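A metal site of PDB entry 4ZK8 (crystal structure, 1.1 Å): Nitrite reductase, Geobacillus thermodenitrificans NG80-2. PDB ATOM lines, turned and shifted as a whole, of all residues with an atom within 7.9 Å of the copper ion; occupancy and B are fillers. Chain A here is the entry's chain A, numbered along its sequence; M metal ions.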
ATOM      1  N   ALA A  47      17.711   5.717 -32.584  1.00  0.00           N
ATOM      2  CA  ALA A  47      17.575   5.609 -31.136  1.00  0.00           C
ATOM      3  C   ALA A  47      18.767   6.415 -30.574  1.00  0.00           C
ATOM      4  O   ALA A  47      19.921   6.155 -30.979  1.00  0.00           O
ATOM      5  CB  ALA A  47      17.681   4.153 -30.682  1.00  0.00           C
ATOM      6  N   ILE A  49      20.230   9.126 -27.084  1.00  0.00           N
ATOM      7  CA  ILE A  49      20.162   9.484 -25.646  1.00  0.00           C
ATOM      8  C   ILE A  49      20.241  10.986 -25.582  1.00  0.00           C
ATOM      9  O   ILE A  49      21.289  11.583 -25.986  1.00  0.00           O
ATOM     10  CB  ILE A  49      21.343   8.820 -24.895  1.00  0.00           C
ATOM     11  CG1 ILE A  49      21.290   7.335 -25.034  1.00  0.00           C
ATOM     12  CG2 ILE A  49      21.339   9.256 -23.412  1.00  0.00           C
ATOM     13  CD1 ILE A  49      19.955   6.609 -24.632  1.00  0.00           C
ATOM     14  N   TRP A  63      15.863   8.093 -23.095  1.00  0.00           N
ATOM     15  CA  TRP A  63      16.045   7.170 -24.226  1.00  0.00           C
ATOM     16  C   TRP A  63      15.032   7.524 -25.208  1.00  0.00           C
ATOM     17  O   TRP A  63      13.833   7.539 -24.853  1.00  0.00           O
ATOM     18  CB  TRP A  63      15.955   5.737 -23.718  1.00  0.00           C
ATOM     19  CG  TRP A  63      16.867   5.287 -22.634  1.00  0.00           C
ATOM     20  CD1 TRP A  63      17.747   5.992 -21.952  1.00  0.00           C
ATOM     21  CD2 TRP A  63      17.017   3.925 -22.183  1.00  0.00           C
ATOM     22  NE1 TRP A  63      18.426   5.168 -21.041  1.00  0.00           N
ATOM     23  CE2 TRP A  63      17.940   3.914 -21.178  1.00  0.00           C
ATOM     24  CE3 TRP A  63      16.317   2.760 -22.527  1.00  0.00           C
ATOM     25  CZ2 TRP A  63      18.331   2.739 -20.537  1.00  0.00           C
ATOM     26  CZ3 TRP A  63      16.689   1.576 -21.831  1.00  0.00           C
ATOM     27  CH2 TRP A  63      17.637   1.593 -20.861  1.00  0.00           C
ATOM     28  N   THR A  64      15.408   7.813 -26.438  1.00  0.00           N
ATOM     29  CA  THR A  64      14.506   8.439 -27.374  1.00  0.00           C
ATOM     30  C   THR A  64      14.610   7.863 -28.801  1.00  0.00           C
ATOM     31  O   THR A  64      15.676   7.278 -29.124  1.00  0.00           O
ATOM     32  CB  THR A  64      14.754   9.941 -27.551  1.00  0.00           C
ATOM     33  OG1 THR A  64      15.924  10.203 -28.290  1.00  0.00           O
ATOM     34  CG2 THR A  64      14.830  10.655 -26.190  1.00  0.00           C
ATOM     35  N   PHE A  65      13.590   8.112 -29.576  1.00  0.00           N
ATOM     36  CA  PHE A  65      13.676   8.144 -31.017  1.00  0.00           C
ATOM     37  C   PHE A  65      13.956   9.568 -31.460  1.00  0.00           C
ATOM     38  O   PHE A  65      13.178  10.460 -31.147  1.00  0.00           O
ATOM     39  CB  PHE A  65      12.433   7.617 -31.634  1.00  0.00           C
ATOM     40  CG  PHE A  65      12.176   6.156 -31.272  1.00  0.00           C
ATOM     41  CD1 PHE A  65      12.905   5.133 -31.898  1.00  0.00           C
ATOM     42  CD2 PHE A  65      11.177   5.807 -30.357  1.00  0.00           C
ATOM     43  CE1 PHE A  65      12.635   3.780 -31.597  1.00  0.00           C
ATOM     44  CE2 PHE A  65      10.933   4.463 -30.104  1.00  0.00           C
ATOM     45  CZ  PHE A  65      11.657   3.443 -30.700  1.00  0.00           C
ATOM     46  N   LEU A  86      16.036   1.695 -38.367  1.00  0.00           N
ATOM     47  CA  LEU A  86      16.464   2.215 -37.111  1.00  0.00           C
ATOM     48  C   LEU A  86      17.979   2.250 -37.029  1.00  0.00           C
ATOM     49  O   LEU A  86      18.621   1.178 -37.168  1.00  0.00           O
ATOM     50  CB  LEU A  86      15.904   1.393 -35.901  1.00  0.00           C
ATOM     51  CG  LEU A  86      16.235   1.942 -34.504  1.00  0.00           C
ATOM     52  CD1 LEU A  86      15.558   3.291 -34.253  1.00  0.00           C
ATOM     53  CD2 LEU A  86      15.833   0.922 -33.460  1.00  0.00           C
ATOM     54  N   ASN A  88      20.825   2.834 -34.428  1.00  0.00           N
ATOM     55  CA  ASN A  88      20.960   2.908 -32.994  1.00  0.00           C
ATOM     56  C   ASN A  88      22.259   3.662 -32.645  1.00  0.00           C
ATOM     57  O   ASN A  88      23.359   3.171 -32.899  1.00  0.00           O
ATOM     58  CB  ASN A  88      21.005   1.481 -32.389  1.00  0.00           C
ATOM     59  CG  ASN A  88      21.008   1.546 -30.898  1.00  0.00           C
ATOM     60  OD1 ASN A  88      20.985   2.638 -30.322  1.00  0.00           O
ATOM     61  ND2 ASN A  88      21.115   0.408 -30.261  1.00  0.00           N
ATOM     62  N   ASP A  90      22.794   4.767 -29.476  1.00  0.00           N
ATOM     63  CA  ASP A  90      23.107   4.513 -28.086  1.00  0.00           C
ATOM     64  C   ASP A  90      24.415   3.693 -28.049  1.00  0.00           C
ATOM     65  O   ASP A  90      24.558   2.699 -28.754  1.00  0.00           O
ATOM     66  CB  ASP A  90      21.968   3.677 -27.463  1.00  0.00           C
ATOM     67  CG  ASP A  90      22.050   3.531 -25.969  1.00  0.00           C
ATOM     68  OD1 ASP A  90      23.207   3.297 -25.410  1.00  0.00           O
ATOM     69  OD2 ASP A  90      20.987   3.513 -25.309  1.00  0.00           O
ATOM     70  N   VAL A  93      23.233   0.311 -25.225  1.00  0.00           N
ATOM     71  CA  VAL A  93      21.968  -0.445 -25.098  1.00  0.00           C
ATOM     72  C   VAL A  93      21.398  -0.712 -26.449  1.00  0.00           C
ATOM     73  O   VAL A  93      21.259   0.215 -27.265  1.00  0.00           O
ATOM     74  CB  VAL A  93      20.963   0.316 -24.216  1.00  0.00           C
ATOM     75  CG1 VAL A  93      19.747  -0.514 -23.879  1.00  0.00           C
ATOM     76  CG2 VAL A  93      21.541   0.840 -22.967  1.00  0.00           C
ATOM     77  N   PRO A  94      20.953  -1.959 -26.736  1.00  0.00           N
ATOM     78  CA  PRO A  94      20.223  -2.251 -27.955  1.00  0.00           C
ATOM     79  C   PRO A  94      18.808  -1.587 -27.921  1.00  0.00           C
ATOM     80  O   PRO A  94      18.274  -1.391 -26.816  1.00  0.00           O
ATOM     81  CB  PRO A  94      20.072  -3.778 -27.985  1.00  0.00           C
ATOM     82  CG  PRO A  94      21.103  -4.286 -27.019  1.00  0.00           C
ATOM     83  CD  PRO A  94      21.189  -3.188 -25.926  1.00  0.00           C
ATOM     84  N   HIS A  95      18.263  -1.320 -29.084  1.00  0.00           N
ATOM     85  CA  HIS A  95      16.904  -0.765 -29.192  1.00  0.00           C
ATOM     86  C   HIS A  95      16.225  -1.377 -30.366  1.00  0.00           C
ATOM     87  O   HIS A  95      16.825  -2.021 -31.274  1.00  0.00           O
ATOM     88  CB  HIS A  95      16.921   0.784 -29.287  1.00  0.00           C
ATOM     89  CG  HIS A  95      17.506   1.421 -28.090  1.00  0.00           C
ATOM     90  ND1 HIS A  95      16.864   1.473 -26.873  1.00  0.00           N
ATOM     91  CD2 HIS A  95      18.683   2.051 -27.917  1.00  0.00           C
ATOM     92  CE1 HIS A  95      17.644   2.044 -26.012  1.00  0.00           C
ATOM     93  NE2 HIS A  95      18.748   2.421 -26.600  1.00  0.00           N
ATOM     94  N   SER A  96      14.909  -1.167 -30.471  1.00  0.00           N
ATOM     95  CA  SER A  96      14.061  -1.778 -31.456  1.00  0.00           C
ATOM     96  C   SER A  96      12.852  -0.879 -31.761  1.00  0.00           C
ATOM     97  O   SER A  96      12.692   0.157 -31.031  1.00  0.00           O
ATOM     98  CB  SER A  96      13.618  -3.180 -31.037  1.00  0.00           C
ATOM     99  OG  SER A  96      12.922  -3.108 -29.803  1.00  0.00           O
ATOM    100  N   MET A  97      12.003  -1.307 -32.641  1.00  0.00           N
ATOM    101  CA  MET A  97      10.796  -0.555 -32.924  1.00  0.00           C
ATOM    102  C   MET A  97       9.622  -1.499 -33.104  1.00  0.00           C
ATOM    103  O   MET A  97       9.659  -2.452 -33.921  1.00  0.00           O
ATOM    104  CB  MET A  97      10.946   0.245 -34.226  1.00  0.00           C
ATOM    105  CG  MET A  97       9.705   0.971 -34.686  1.00  0.00           C
ATOM    106  SD  MET A  97       8.998   2.163 -33.534  1.00  0.00           S
ATOM    107  CE  MET A  97       9.992   3.566 -33.963  1.00  0.00           C
ATOM    108  N   ASP A 112      16.018  -6.460 -32.001  1.00  0.00           N
ATOM    109  CA  ASP A 112      17.028  -5.502 -31.585  1.00  0.00           C
ATOM    110  C   ASP A 112      17.998  -5.112 -32.674  1.00  0.00           C
ATOM    111  O   ASP A 112      18.448  -5.939 -33.460  1.00  0.00           O
ATOM    112  CB  ASP A 112      17.759  -6.030 -30.362  1.00  0.00           C
ATOM    113  CG  ASP A 112      16.864  -6.139 -29.096  1.00  0.00           C
ATOM    114  OD1 ASP A 112      15.781  -5.532 -29.031  1.00  0.00           O
ATOM    115  OD2 ASP A 112      17.238  -6.833 -28.152  1.00  0.00           O
ATOM    116  N   VAL A 113      18.410  -3.861 -32.592  1.00  0.00           N
ATOM    117  CA  VAL A 113      19.519  -3.255 -33.356  1.00  0.00           C
ATOM    118  C   VAL A 113      20.534  -2.888 -32.374  1.00  0.00           C
ATOM    119  O   VAL A 113      20.267  -2.153 -31.368  1.00  0.00           O
ATOM    120  CB  VAL A 113      18.995  -2.073 -34.148  1.00  0.00           C
ATOM    121  CG1 VAL A 113      20.153  -1.398 -34.892  1.00  0.00           C
ATOM    122  CG2 VAL A 113      17.870  -2.434 -35.053  1.00  0.00           C
ATOM    123  N   HIS A 134       6.672   2.215 -30.120  1.00  0.00           N
ATOM    124  CA  HIS A 134       7.582   2.213 -28.989  1.00  0.00           C
ATOM    125  C   HIS A 134       8.709   1.232 -29.205  1.00  0.00           C
ATOM    126  O   HIS A 134       8.604   0.328 -30.038  1.00  0.00           O
ATOM    127  CB  HIS A 134       6.815   1.873 -27.695  1.00  0.00           C
ATOM    128  CG  HIS A 134       6.120   0.525 -27.720  1.00  0.00           C
ATOM    129  ND1 HIS A 134       6.737  -0.638 -27.328  1.00  0.00           N
ATOM    130  CD2 HIS A 134       4.835   0.187 -28.007  1.00  0.00           C
ATOM    131  CE1 HIS A 134       5.864  -1.648 -27.400  1.00  0.00           C
ATOM    132  NE2 HIS A 134       4.696  -1.182 -27.799  1.00  0.00           N
ATOM    133  N   CYS A 135       9.775   1.411 -28.458  1.00  0.00           N
ATOM    134  CA  CYS A 135      10.827   0.398 -28.380  1.00  0.00           C
ATOM    135  C   CYS A 135      10.253  -0.902 -27.861  1.00  0.00           C
ATOM    136  O   CYS A 135       9.489  -0.880 -26.892  1.00  0.00           O
ATOM    137  CB  CYS A 135      11.994   0.926 -27.649  1.00  0.00           C
ATOM    138  SG  CYS A 135      13.381  -0.228 -27.510  1.00  0.00           S
ATOM    139  N   GLY A 136      10.730  -2.042 -28.390  1.00  0.00           N
ATOM    140  CA  GLY A 136      10.314  -3.323 -27.975  1.00  0.00           C
ATOM    141  C   GLY A 136      11.385  -4.181 -27.367  1.00  0.00           C
ATOM    142  O   GLY A 136      11.283  -5.422 -27.366  1.00  0.00           O
ATOM    143  N   THR A 137      12.442  -3.560 -26.837  1.00  0.00           N
ATOM    144  CA  THR A 137      13.550  -4.320 -26.305  1.00  0.00           C
ATOM    145  C   THR A 137      13.314  -4.635 -24.877  1.00  0.00           C
ATOM    146  O   THR A 137      12.853  -3.807 -24.068  1.00  0.00           O
ATOM    147  CB  THR A 137      14.837  -3.419 -26.459  1.00  0.00           C
ATOM    148  OG1 THR A 137      15.022  -3.223 -27.876  1.00  0.00           O
ATOM    149  CG2 THR A 137      16.063  -4.078 -25.888  1.00  0.00           C
ATOM    150  N   LYS A 138      13.641  -5.874 -24.438  1.00  0.00           N
ATOM    151  CA  LYS A 138      13.452  -6.297 -23.079  1.00  0.00           C
ATOM    152  C   LYS A 138      14.390  -5.552 -22.151  1.00  0.00           C
ATOM    153  O   LYS A 138      15.616  -5.491 -22.456  1.00  0.00           O
ATOM    154  CB  LYS A 138      13.718  -7.820 -22.971  1.00  0.00           C
ATOM    155  CG  LYS A 138      13.511  -8.417 -21.598  1.00  0.00           C
ATOM    156  CD  LYS A 138      13.719  -9.929 -21.585  1.00  0.00           C
ATOM    157  CE  LYS A 138      13.101 -10.507 -20.344  1.00  0.00           C
ATOM    158  NZ  LYS A 138      13.122 -11.988 -20.427  1.00  0.00           N
ATOM    159  N   PRO A 139      13.999  -5.089 -20.935  1.00  0.00           N
ATOM    160  CA  PRO A 139      12.595  -5.025 -20.468  1.00  0.00           C
ATOM    161  C   PRO A 139      11.843  -3.897 -21.160  1.00  0.00           C
ATOM    162  O   PRO A 139      12.297  -2.712 -21.057  1.00  0.00           O
ATOM    163  CB  PRO A 139      12.783  -4.784 -19.010  1.00  0.00           C
ATOM    164  CG  PRO A 139      14.194  -4.751 -18.715  1.00  0.00           C
ATOM    165  CD  PRO A 139      14.932  -4.580 -19.987  1.00  0.00           C
ATOM    166  N   VAL A 140      10.726  -4.205 -21.767  1.00  0.00           N
ATOM    167  CA  VAL A 140      10.051  -3.160 -22.542  1.00  0.00           C
ATOM    168  C   VAL A 140       9.575  -2.026 -21.613  1.00  0.00           C
ATOM    169  O   VAL A 140       9.650  -0.851 -22.027  1.00  0.00           O
ATOM    170  CB  VAL A 140       8.857  -3.781 -23.335  1.00  0.00           C
ATOM    171  CG1 VAL A 140       7.995  -2.726 -23.985  1.00  0.00           C
ATOM    172  CG2 VAL A 140       9.416  -4.736 -24.382  1.00  0.00           C
ATOM    173  N   GLN A 142      11.172  -0.717 -19.247  1.00  0.00           N
ATOM    174  CA  GLN A 142      12.303   0.201 -19.069  1.00  0.00           C
ATOM    175  C   GLN A 142      12.448   1.126 -20.259  1.00  0.00           C
ATOM    176  O   GLN A 142      12.718   2.335 -20.136  1.00  0.00           O
ATOM    177  CB  GLN A 142      13.567  -0.625 -18.801  1.00  0.00           C
ATOM    178  CG  GLN A 142      14.789   0.247 -18.514  1.00  0.00           C
ATOM    179  CD  GLN A 142      15.952  -0.584 -18.150  1.00  0.00           C
ATOM    180  OE1 GLN A 142      16.051  -1.790 -18.444  1.00  0.00           O
ATOM    181  NE2 GLN A 142      16.919   0.032 -17.559  1.00  0.00           N
ATOM    182  N   HIS A 143      12.368   0.517 -21.468  1.00  0.00           N
ATOM    183  CA  HIS A 143      12.584   1.288 -22.679  1.00  0.00           C
ATOM    184  C   HIS A 143      11.475   2.278 -22.891  1.00  0.00           C
ATOM    185  O   HIS A 143      11.707   3.476 -23.240  1.00  0.00           O
ATOM    186  CB  HIS A 143      12.794   0.401 -23.873  1.00  0.00           C
ATOM    187  CG  HIS A 143      14.082  -0.338 -23.838  1.00  0.00           C
ATOM    188  ND1 HIS A 143      15.135   0.006 -24.693  1.00  0.00           N
ATOM    189  CD2 HIS A 143      14.525  -1.339 -23.018  1.00  0.00           C
ATOM    190  CE1 HIS A 143      16.151  -0.767 -24.394  1.00  0.00           C
ATOM    191  NE2 HIS A 143      15.832  -1.586 -23.419  1.00  0.00           N
ATOM    192  N   ILE A 144      10.206   1.893 -22.670  1.00  0.00           N
ATOM    193  CA  ILE A 144       9.121   2.836 -22.782  1.00  0.00           C
ATOM    194  C   ILE A 144       9.239   3.919 -21.713  1.00  0.00           C
ATOM    195  O   ILE A 144       9.145   5.145 -22.006  1.00  0.00           O
ATOM    196  CB  ILE A 144       7.718   2.150 -22.703  1.00  0.00           C
ATOM    197  CG1 ILE A 144       7.572   1.164 -23.858  1.00  0.00           C
ATOM    198  CG2 ILE A 144       6.647   3.198 -22.730  1.00  0.00           C
ATOM    199  CD1 ILE A 144       6.239   0.368 -23.803  1.00  0.00           C
ATOM    200  N   ASN A 146      11.647   5.145 -20.118  1.00  0.00           N
ATOM    201  CA  ASN A 146      12.758   6.064 -20.349  1.00  0.00           C
ATOM    202  C   ASN A 146      12.526   7.032 -21.532  1.00  0.00           C
ATOM    203  O   ASN A 146      13.361   7.946 -21.669  1.00  0.00           O
ATOM    204  CB  ASN A 146      14.073   5.345 -20.453  1.00  0.00           C
ATOM    205  CG  ASN A 146      14.655   4.921 -19.167  1.00  0.00           C
ATOM    206  OD1 ASN A 146      14.534   5.616 -18.084  1.00  0.00           O
ATOM    207  ND2 ASN A 146      15.386   3.812 -19.143  1.00  0.00           N
ATOM    208  N   GLY A 147      11.487   6.846 -22.301  1.00  0.00           N
ATOM    209  CA  GLY A 147      11.057   7.774 -23.306  1.00  0.00           C
ATOM    210  C   GLY A 147      10.849   7.238 -24.701  1.00  0.00           C
ATOM    211  O   GLY A 147      10.491   8.028 -25.562  1.00  0.00           O
ATOM    212  N   MET A 148      10.947   5.913 -24.908  1.00  0.00           N
ATOM    213  CA  MET A 148      10.892   5.408 -26.288  1.00  0.00           C
ATOM    214  C   MET A 148       9.472   5.023 -26.680  1.00  0.00           C
ATOM    215  O   MET A 148       9.103   3.844 -26.763  1.00  0.00           O
ATOM    216  CB  MET A 148      11.847   4.210 -26.414  1.00  0.00           C
ATOM    217  CG  MET A 148      13.267   4.595 -26.021  1.00  0.00           C
ATOM    218  SD  MET A 148      14.581   3.466 -26.522  1.00  0.00           S
ATOM    219  CE  MET A 148      14.656   3.874 -28.226  1.00  0.00           C
HETATM  220 CU    CU M   1      14.943   0.887 -26.509  1.00  0.00          CU
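N of Val 113 is in hydrogen-bond range of O of His 95, at 2.8 Å.
The side-chain sulfur (SG) of Cys 135 sits close to the side-chain hydroxyl (OG1) of Thr 137 (3.4 Å).
A ring nitrogen (NE2) of His 95 is in hydrogen-bond range of the side-chain carboxylate (OD2) of Asp 90, 2.8 Å away.
N of Met 148 sits close to O of Trp 63.
The side-chain sulfur of Cys 135 lies close to the backbone NH of Ser 96, at 3.5 Å.
O of Val 93 sits close to NE2 of His 95 (3.4 Å).
Of the 28 residues printed, 4 come within 4 Å of the copper ion.
The copper ion is bound by a ring nitrogen (ND1) of His 143 (2.0 Å), a ring nitrogen (ND1) of His 95 (2.0 Å), the side-chain sulfur (SG) of Cys 135 (2.2 Å) and the side-chain sulfur (SD) of Met 148 (2.6 Å).
The copper ion has four donor atoms within binding distance.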
